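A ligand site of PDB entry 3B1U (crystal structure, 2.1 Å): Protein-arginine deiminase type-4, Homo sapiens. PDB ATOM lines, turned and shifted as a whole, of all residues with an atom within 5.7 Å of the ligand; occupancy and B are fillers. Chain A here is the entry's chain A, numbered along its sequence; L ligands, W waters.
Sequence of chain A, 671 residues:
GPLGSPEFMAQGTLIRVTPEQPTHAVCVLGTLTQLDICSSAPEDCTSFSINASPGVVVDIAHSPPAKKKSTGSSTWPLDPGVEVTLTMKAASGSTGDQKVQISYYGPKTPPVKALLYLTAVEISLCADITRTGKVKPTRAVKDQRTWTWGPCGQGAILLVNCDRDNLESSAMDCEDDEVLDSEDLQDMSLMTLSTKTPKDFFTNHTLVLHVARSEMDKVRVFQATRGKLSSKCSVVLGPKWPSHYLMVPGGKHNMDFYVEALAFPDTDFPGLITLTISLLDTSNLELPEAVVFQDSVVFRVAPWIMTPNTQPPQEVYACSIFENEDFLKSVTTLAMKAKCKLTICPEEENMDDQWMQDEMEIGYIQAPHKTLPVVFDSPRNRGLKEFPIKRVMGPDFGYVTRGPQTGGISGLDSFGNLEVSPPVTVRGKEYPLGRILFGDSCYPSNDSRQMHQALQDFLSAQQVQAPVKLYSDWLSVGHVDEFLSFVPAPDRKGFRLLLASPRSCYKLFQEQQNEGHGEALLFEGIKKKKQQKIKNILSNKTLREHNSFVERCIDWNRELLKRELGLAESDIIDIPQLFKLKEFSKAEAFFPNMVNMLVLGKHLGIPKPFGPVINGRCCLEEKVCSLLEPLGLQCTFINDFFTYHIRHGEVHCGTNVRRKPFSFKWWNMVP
A carbon (C10) of the ligand is bonded to the side-chain sulfur of Cys 653, at 1.8 Å. An oxygen (O3) of the ligand sits at hydrogen-bond distance from the guanidinium group of Arg 382, 2.7 Å away. The indole nitrogen of Trp 355 lies within hydrogen-bond range of an oxygen (O2) of the ligand. A nitrogen (N2) of the ligand is in salt-bridge range of the side-chain carboxylate (OD1) of Asp 358 (2.9 Å). A nitrogen (N2) of the ligand lies within hydrogen-bond range of a ring nitrogen (ND1) of His 479 (3.0 Å). A nitrogen (N4) of the ligand sits at hydrogen-bond distance from the backbone carbonyl oxygen (O) of Arg 647, 3.1 Å away. N2 of the ligand lies within salt-bridge range of OD1 of Asp 481.
The backbone NH (N) of Gln 357 sits at hydrogen-bond distance from the backbone carbonyl oxygen (O) of Cys 653, 3.1 Å away. The guanidinium group (NH2) of Arg 380 sits at hydrogen-bond distance from the backbone carbonyl oxygen (O) of Trp 355 (3.0 Å). N of Trp 355 lies within hydrogen-bond range of OD1 of Asp 353 (3.3 Å). The guanidinium group (NE) of Arg 647 is in hydrogen-bond range of the side-chain amide oxygen (OE1) of Gln 354, 3.1 Å away. ND2 of Asn 596 sits at hydrogen-bond distance from O of Asp 481 (3.1 Å). The backbone NH (N) of Asp 481 lies close to the backbone carbonyl oxygen (O) of Gly 416 (3.4 Å). The side-chain carboxylate of Asp 481 sits at hydrogen-bond distance from a ring nitrogen (ND1) of His 652. The side-chain amide oxygen of Asn 596 is in hydrogen-bond range of the backbone NH of His 652, at 3.1 Å.
CG1 of Val 477 touches C7 of the ligand (3.3 Å). Asn 596 touches the ligand. His 648 touches the ligand (O to C9, 3.3 Å). Hydrophobic or aromatic side chains within 4 Å of the ligand: Trp 355, Val 477, His 479 and His 648.
Water W4 lies within hydrogen-bond range of an oxygen (O2) of the ligand (2.7 Å), the backbone carbonyl oxygen (O) of Asp 352 (2.8 Å), the side-chain amide oxygen (OE1) of Gln 354 (2.9 Å) and the indole nitrogen (NE1) of Trp 355 (3.5 Å). Water W2 lies within hydrogen-bond range of OD2 of Asp 358 (2.5 Å), NH1 of Arg 380 (2.7 Å), O3 of the ligand (2.8 Å) and NH2 of Arg 382 (3.0 Å). Water W5 bridges NH2 of Arg 382 and O3 of the ligand. Water W3 bridges NH2 of Arg 647 (2.7 Å) and O1 of the ligand (3.4 Å).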
ATOM      1  N   ASP A 352      13.950 -12.783  16.948  1.00  0.00           N
ATOM      2  CA  ASP A 352      13.733 -11.873  18.085  1.00  0.00           C
ATOM      3  C   ASP A 352      13.870 -10.380  17.753  1.00  0.00           C
ATOM      4  O   ASP A 352      14.108  -9.559  18.642  1.00  0.00           O
ATOM      5  CB  ASP A 352      14.642 -12.245  19.270  1.00  0.00           C
ATOM      6  CG  ASP A 352      14.469 -13.698  19.701  1.00  0.00           C
ATOM      7  OD1 ASP A 352      15.338 -14.194  20.451  1.00  0.00           O
ATOM      8  OD2 ASP A 352      13.471 -14.340  19.297  1.00  0.00           O
ATOM      9  N   ASP A 353      13.696 -10.036  16.472  1.00  0.00           N
ATOM     10  CA  ASP A 353      13.707  -8.640  16.023  1.00  0.00           C
ATOM     11  C   ASP A 353      12.273  -8.130  15.919  1.00  0.00           C
ATOM     12  O   ASP A 353      11.522  -8.522  15.023  1.00  0.00           O
ATOM     13  CB  ASP A 353      14.418  -8.523  14.676  1.00  0.00           C
ATOM     14  CG  ASP A 353      14.510  -7.094  14.169  1.00  0.00           C
ATOM     15  OD1 ASP A 353      14.242  -6.139  14.933  1.00  0.00           O
ATOM     16  OD2 ASP A 353      14.856  -6.908  12.977  1.00  0.00           O
ATOM     17  N   GLN A 354      11.891  -7.256  16.855  1.00  0.00           N
ATOM     18  CA  GLN A 354      10.512  -6.778  16.976  1.00  0.00           C
ATOM     19  C   GLN A 354      10.243  -5.463  16.229  1.00  0.00           C
ATOM     20  O   GLN A 354       9.100  -5.004  16.181  1.00  0.00           O
ATOM     21  CB  GLN A 354      10.154  -6.596  18.451  1.00  0.00           C
ATOM     22  CG  GLN A 354      10.830  -5.406  19.121  1.00  0.00           C
ATOM     23  CD  GLN A 354      10.872  -5.524  20.632  1.00  0.00           C
ATOM     24  OE1 GLN A 354      11.903  -5.862  21.204  1.00  0.00           O
ATOM     25  NE2 GLN A 354       9.744  -5.252  21.274  1.00  0.00           N
ATOM     26  N   TRP A 355      11.279  -4.862  15.649  1.00  0.00           N
ATOM     27  CA  TRP A 355      11.177  -3.506  15.113  1.00  0.00           C
ATOM     28  C   TRP A 355      10.789  -3.502  13.635  1.00  0.00           C
ATOM     29  O   TRP A 355      11.623  -3.292  12.745  1.00  0.00           O
ATOM     30  CB  TRP A 355      12.488  -2.753  15.348  1.00  0.00           C
ATOM     31  CG  TRP A 355      12.929  -2.847  16.780  1.00  0.00           C
ATOM     32  CD1 TRP A 355      14.012  -3.532  17.250  1.00  0.00           C
ATOM     33  CD2 TRP A 355      12.277  -2.278  17.917  1.00  0.00           C
ATOM     34  NE1 TRP A 355      14.088  -3.411  18.623  1.00  0.00           N
ATOM     35  CE2 TRP A 355      13.025  -2.648  19.059  1.00  0.00           C
ATOM     36  CE3 TRP A 355      11.140  -1.483  18.087  1.00  0.00           C
ATOM     37  CZ2 TRP A 355      12.672  -2.253  20.346  1.00  0.00           C
ATOM     38  CZ3 TRP A 355      10.787  -1.088  19.374  1.00  0.00           C
ATOM     39  CH2 TRP A 355      11.553  -1.466  20.484  1.00  0.00           C
ATOM     40  N   GLN A 357       9.088  -1.410  11.993  1.00  0.00           N
ATOM     41  CA  GLN A 357       9.248  -0.086  11.389  1.00  0.00           C
ATOM     42  C   GLN A 357      10.591   0.074  10.676  1.00  0.00           C
ATOM     43  O   GLN A 357      10.691   0.779   9.674  1.00  0.00           O
ATOM     44  CB  GLN A 357       9.133   0.984  12.477  1.00  0.00           C
ATOM     45  CG  GLN A 357       9.360   2.433  12.018  1.00  0.00           C
ATOM     46  CD  GLN A 357       8.327   2.919  11.022  1.00  0.00           C
ATOM     47  OE1 GLN A 357       8.599   3.829  10.236  1.00  0.00           O
ATOM     48  NE2 GLN A 357       7.129   2.341  11.058  1.00  0.00           N
ATOM     49  N   ASP A 358      11.612  -0.577  11.206  1.00  0.00           N
ATOM     50  CA  ASP A 358      12.994  -0.192  10.907  1.00  0.00           C
ATOM     51  C   ASP A 358      13.621  -0.885   9.695  1.00  0.00           C
ATOM     52  O   ASP A 358      14.470  -0.288   9.034  1.00  0.00           O
ATOM     53  CB  ASP A 358      13.853  -0.413  12.156  1.00  0.00           C
ATOM     54  CG  ASP A 358      13.492   0.536  13.287  1.00  0.00           C
ATOM     55  OD1 ASP A 358      12.898   1.614  13.018  1.00  0.00           O
ATOM     56  OD2 ASP A 358      13.802   0.212  14.441  1.00  0.00           O
ATOM     57  N   ARG A 380      20.003  -2.112   7.307  1.00  0.00           N
ATOM     58  CA  ARG A 380      20.306  -2.430   8.722  1.00  0.00           C
ATOM     59  C   ARG A 380      20.447  -3.940   8.956  1.00  0.00           C
ATOM     60  O   ARG A 380      21.210  -4.352   9.829  1.00  0.00           O
ATOM     61  CB  ARG A 380      19.276  -1.799   9.680  1.00  0.00           C
ATOM     62  CG  ARG A 380      17.917  -2.470   9.757  1.00  0.00           C
ATOM     63  CD  ARG A 380      17.398  -2.509  11.197  1.00  0.00           C
ATOM     64  NE  ARG A 380      16.155  -3.274  11.308  1.00  0.00           N
ATOM     65  CZ  ARG A 380      15.595  -3.646  12.456  1.00  0.00           C
ATOM     66  NH1 ARG A 380      16.138  -3.339  13.627  1.00  0.00           N
ATOM     67  NH2 ARG A 380      14.461  -4.337  12.431  1.00  0.00           N
ATOM     68  N   ARG A 382      19.010  -6.574  10.366  1.00  0.00           N
ATOM     69  CA  ARG A 382      18.931  -7.163  11.689  1.00  0.00           C
ATOM     70  C   ARG A 382      18.161  -8.499  11.577  1.00  0.00           C
ATOM     71  O   ARG A 382      18.185  -9.129  10.525  1.00  0.00           O
ATOM     72  CB  ARG A 382      18.269  -6.185  12.676  1.00  0.00           C
ATOM     73  CG  ARG A 382      18.918  -6.166  14.052  1.00  0.00           C
ATOM     74  CD  ARG A 382      19.914  -5.018  14.210  1.00  0.00           C
ATOM     75  NE  ARG A 382      19.264  -3.793  14.664  1.00  0.00           N
ATOM     76  CZ  ARG A 382      18.821  -3.577  15.908  1.00  0.00           C
ATOM     77  NH1 ARG A 382      18.960  -4.503  16.848  1.00  0.00           N
ATOM     78  NH2 ARG A 382      18.247  -2.430  16.209  1.00  0.00           N
ATOM     79  N   SER A 414      17.998   2.860   9.872  1.00  0.00           N
ATOM     80  CA  SER A 414      16.722   2.228  10.205  1.00  0.00           C
ATOM     81  C   SER A 414      15.587   3.148   9.775  1.00  0.00           C
ATOM     82  O   SER A 414      15.655   4.354   9.989  1.00  0.00           O
ATOM     83  CB  SER A 414      16.630   1.958  11.702  1.00  0.00           C
ATOM     84  OG  SER A 414      17.592   1.000  12.118  1.00  0.00           O
ATOM     85  N   GLY A 416      12.614   3.870  10.694  1.00  0.00           N
ATOM     86  CA  GLY A 416      11.927   4.770  11.619  1.00  0.00           C
ATOM     87  C   GLY A 416      12.451   6.187  11.437  1.00  0.00           C
ATOM     88  O   GLY A 416      11.788   7.159  11.792  1.00  0.00           O
ATOM     89  N   VAL A 477      18.460   6.630  19.845  1.00  0.00           N
ATOM     90  CA  VAL A 477      18.130   5.823  18.678  1.00  0.00           C
ATOM     91  C   VAL A 477      18.323   6.652  17.402  1.00  0.00           C
ATOM     92  O   VAL A 477      18.934   6.184  16.448  1.00  0.00           O
ATOM     93  CB  VAL A 477      16.685   5.284  18.767  1.00  0.00           C
ATOM     94  CG1 VAL A 477      16.331   4.489  17.533  1.00  0.00           C
ATOM     95  CG2 VAL A 477      16.511   4.441  20.035  1.00  0.00           C
ATOM     96  N   HIS A 479      15.870   8.712  15.490  1.00  0.00           N
ATOM     97  CA  HIS A 479      14.863   8.591  14.429  1.00  0.00           C
ATOM     98  C   HIS A 479      13.876   9.749  14.478  1.00  0.00           C
ATOM     99  O   HIS A 479      13.426  10.133  15.554  1.00  0.00           O
ATOM    100  CB  HIS A 479      14.109   7.281  14.577  1.00  0.00           C
ATOM    101  CG  HIS A 479      14.960   6.062  14.387  1.00  0.00           C
ATOM    102  ND1 HIS A 479      14.439   4.785  14.410  1.00  0.00           N
ATOM    103  CD2 HIS A 479      16.284   5.925  14.141  1.00  0.00           C
ATOM    104  CE1 HIS A 479      15.410   3.912  14.210  1.00  0.00           C
ATOM    105  NE2 HIS A 479      16.539   4.579  14.037  1.00  0.00           N
ATOM    106  N   ASP A 481      10.799   9.729  13.754  1.00  0.00           N
ATOM    107  CA  ASP A 481       9.517   9.267  14.312  1.00  0.00           C
ATOM    108  C   ASP A 481       9.473   9.314  15.854  1.00  0.00           C
ATOM    109  O   ASP A 481       8.412   9.176  16.451  1.00  0.00           O
ATOM    110  CB  ASP A 481       9.141   7.862  13.788  1.00  0.00           C
ATOM    111  CG  ASP A 481       9.957   6.734  14.430  1.00  0.00           C
ATOM    112  OD1 ASP A 481       9.484   5.575  14.364  1.00  0.00           O
ATOM    113  OD2 ASP A 481      11.040   6.989  14.985  1.00  0.00           O
ATOM    114  N   GLU A 482      10.638   9.510  16.477  1.00  0.00           N
ATOM    115  CA  GLU A 482      10.705   9.713  17.926  1.00  0.00           C
ATOM    116  C   GLU A 482      10.232  11.087  18.401  1.00  0.00           C
ATOM    117  O   GLU A 482       9.963  11.255  19.585  1.00  0.00           O
ATOM    118  CB  GLU A 482      12.133   9.504  18.430  1.00  0.00           C
ATOM    119  CG  GLU A 482      12.604   8.079  18.404  1.00  0.00           C
ATOM    120  CD  GLU A 482      13.979   7.945  18.993  1.00  0.00           C
ATOM    121  OE1 GLU A 482      14.089   7.560  20.180  1.00  0.00           O
ATOM    122  OE2 GLU A 482      14.965   8.253  18.280  1.00  0.00           O
ATOM    123  N   ASN A 596       5.095   8.701  19.021  1.00  0.00           N
ATOM    124  CA  ASN A 596       5.477   7.531  18.243  1.00  0.00           C
ATOM    125  C   ASN A 596       4.300   6.562  18.157  1.00  0.00           C
ATOM    126  O   ASN A 596       4.297   5.489  18.775  1.00  0.00           O
ATOM    127  CB  ASN A 596       6.708   6.877  18.898  1.00  0.00           C
ATOM    128  CG  ASN A 596       7.299   5.788  18.045  1.00  0.00           C
ATOM    129  OD1 ASN A 596       6.933   4.617  18.176  1.00  0.00           O
ATOM    130  ND2 ASN A 596       8.238   6.155  17.172  1.00  0.00           N
ATOM    131  N   ILE A 646      10.850  -0.314  27.220  1.00  0.00           N
ATOM    132  CA  ILE A 646      12.103  -0.597  27.945  1.00  0.00           C
ATOM    133  C   ILE A 646      13.263  -0.970  27.012  1.00  0.00           C
ATOM    134  O   ILE A 646      14.410  -0.968  27.435  1.00  0.00           O
ATOM    135  CB  ILE A 646      11.934  -1.687  29.043  1.00  0.00           C
ATOM    136  CG1 ILE A 646      11.483  -3.027  28.448  1.00  0.00           C
ATOM    137  CG2 ILE A 646      10.957  -1.218  30.105  1.00  0.00           C
ATOM    138  CD1 ILE A 646      11.535  -4.165  29.447  1.00  0.00           C
ATOM    139  N   ARG A 647      12.946  -1.305  25.754  1.00  0.00           N
ATOM    140  CA  ARG A 647      13.955  -1.539  24.720  1.00  0.00           C
ATOM    141  C   ARG A 647      14.036  -0.375  23.713  1.00  0.00           C
ATOM    142  O   ARG A 647      14.412  -0.554  22.550  1.00  0.00           O
ATOM    143  CB  ARG A 647      13.676  -2.886  24.037  1.00  0.00           C
ATOM    144  CG  ARG A 647      13.882  -4.072  24.989  1.00  0.00           C
ATOM    145  CD  ARG A 647      12.938  -5.250  24.727  1.00  0.00           C
ATOM    146  NE  ARG A 647      13.519  -6.234  23.808  1.00  0.00           N
ATOM    147  CZ  ARG A 647      13.148  -7.512  23.734  1.00  0.00           C
ATOM    148  NH1 ARG A 647      12.183  -7.993  24.516  1.00  0.00           N
ATOM    149  NH2 ARG A 647      13.740  -8.315  22.858  1.00  0.00           N
ATOM    150  N   HIS A 648      13.671   0.823  24.191  1.00  0.00           N
ATOM    151  CA  HIS A 648      13.900   2.091  23.480  1.00  0.00           C
ATOM    152  C   HIS A 648      13.088   2.271  22.187  1.00  0.00           C
ATOM    153  O   HIS A 648      13.589   2.820  21.213  1.00  0.00           O
ATOM    154  CB  HIS A 648      15.395   2.307  23.236  1.00  0.00           C
ATOM    155  CG  HIS A 648      16.251   2.084  24.442  1.00  0.00           C
ATOM    156  ND1 HIS A 648      16.024   2.726  25.639  1.00  0.00           N
ATOM    157  CD2 HIS A 648      17.320   1.265  24.642  1.00  0.00           C
ATOM    158  CE1 HIS A 648      16.920   2.321  26.533  1.00  0.00           C
ATOM    159  NE2 HIS A 648      17.715   1.440  25.946  1.00  0.00           N
ATOM    160  N   GLY A 649      11.840   1.831  22.205  1.00  0.00           N
ATOM    161  CA  GLY A 649      10.916   2.037  21.081  1.00  0.00           C
ATOM    162  C   GLY A 649       9.465   1.876  21.515  1.00  0.00           C
ATOM    163  O   GLY A 649       9.211   1.450  22.630  1.00  0.00           O
ATOM    164  N   GLU A 650       8.527   2.224  20.640  1.00  0.00           N
ATOM    165  CA  GLU A 650       7.099   2.202  20.989  1.00  0.00           C
ATOM    166  C   GLU A 650       6.253   1.557  19.863  1.00  0.00           C
ATOM    167  O   GLU A 650       6.758   0.741  19.093  1.00  0.00           O
ATOM    168  CB  GLU A 650       6.592   3.612  21.323  1.00  0.00           C
ATOM    169  CG  GLU A 650       7.509   4.455  22.213  1.00  0.00           C
ATOM    170  CD  GLU A 650       7.587   3.975  23.653  1.00  0.00           C
ATOM    171  OE1 GLU A 650       8.524   4.410  24.362  1.00  0.00           O
ATOM    172  OE2 GLU A 650       6.724   3.182  24.092  1.00  0.00           O
ATOM    173  N   HIS A 652       4.750   2.734  17.034  1.00  0.00           N
ATOM    174  CA  HIS A 652       5.154   3.015  15.652  1.00  0.00           C
ATOM    175  C   HIS A 652       6.404   2.210  15.283  1.00  0.00           C
ATOM    176  O   HIS A 652       6.481   1.664  14.188  1.00  0.00           O
ATOM    177  CB  HIS A 652       5.417   4.514  15.441  1.00  0.00           C
ATOM    178  CG  HIS A 652       5.578   4.914  14.011  1.00  0.00           C
ATOM    179  ND1 HIS A 652       6.818   5.169  13.448  1.00  0.00           N
ATOM    180  CD2 HIS A 652       4.678   5.112  13.018  1.00  0.00           C
ATOM    181  CE1 HIS A 652       6.658   5.502  12.180  1.00  0.00           C
ATOM    182  NE2 HIS A 652       5.368   5.479  11.897  1.00  0.00           N
ATOM    183  N   CYS A 653       7.364   2.147  16.210  1.00  0.00           N
ATOM    184  CA  CYS A 653       8.595   1.378  16.004  1.00  0.00           C
ATOM    185  C   CYS A 653       8.337  -0.122  15.809  1.00  0.00           C
ATOM    186  O   CYS A 653       9.018  -0.774  15.021  1.00  0.00           O
ATOM    187  CB  CYS A 653       9.543   1.555  17.192  1.00  0.00           C
ATOM    188  SG  CYS A 653       9.862   3.256  17.665  1.00  0.00           S
HETATM  189  C1  LIG L   1      16.761  -5.203  20.872  1.00  0.00           C
HETATM  190  O1  LIG L   1      17.531  -6.164  20.662  1.00  0.00           O
HETATM  191  O2  LIG L   1      15.715  -5.039  20.200  1.00  0.00           O
HETATM  192  N1  LIG L   1      18.055   0.705  19.119  1.00  0.00           N
HETATM  193  N2  LIG L   1      12.120   3.084  15.370  1.00  0.00           N
HETATM  194  O3  LIG L   1      17.451  -0.064  17.112  1.00  0.00           O
HETATM  195  O4  LIG L   1      17.859  -2.704  19.448  1.00  0.00           O
HETATM  196  C2  LIG L   1      17.528  -3.865  24.324  1.00  0.00           C
HETATM  197  C3  LIG L   1      17.219  -4.728  23.266  1.00  0.00           C
HETATM  198  C4  LIG L   1      17.706  -2.511  24.077  1.00  0.00           C
HETATM  199  C5  LIG L   1      17.090  -4.233  21.970  1.00  0.00           C
HETATM  200  C6  LIG L   1      17.583  -2.023  22.783  1.00  0.00           C
HETATM  201  C7  LIG L   1      14.891   1.650  18.318  1.00  0.00           C
HETATM  202  C8  LIG L   1      13.822   1.513  17.240  1.00  0.00           C
HETATM  203  C9  LIG L   1      14.961   0.463  19.280  1.00  0.00           C
HETATM  204  C10 LIG L   1      11.236   4.353  17.252  1.00  0.00           C
HETATM  205  N3  LIG L   1      12.883   2.585  17.528  1.00  0.00           N
HETATM  206  N4  LIG L   1      16.263  -1.290  20.180  1.00  0.00           N
HETATM  207  C11 LIG L   1      17.245   0.041  18.314  1.00  0.00           C
HETATM  208  C12 LIG L   1      12.126   3.289  16.684  1.00  0.00           C
HETATM  209  C13 LIG L   1      17.151  -2.279  20.347  1.00  0.00           C
HETATM  210  C14 LIG L   1      17.269  -2.878  21.722  1.00  0.00           C
HETATM  211  C15 LIG L   1      16.011  -0.594  18.916  1.00  0.00           C
HETATM  212  O   HOH W   1      18.939   1.707  22.017  1.00  0.00           O
HETATM  213  O   HOH W   2      15.913  -1.017  15.034  1.00  0.00           O
HETATM  214  O   HOH W   3      16.470  -8.527  22.833  1.00  0.00           O
HETATM  215  O   HOH W   4      13.860  -6.801  19.233  1.00  0.00           O
HETATM  216  O   HOH W   5      19.714  -0.733  14.818  1.00  0.00           O
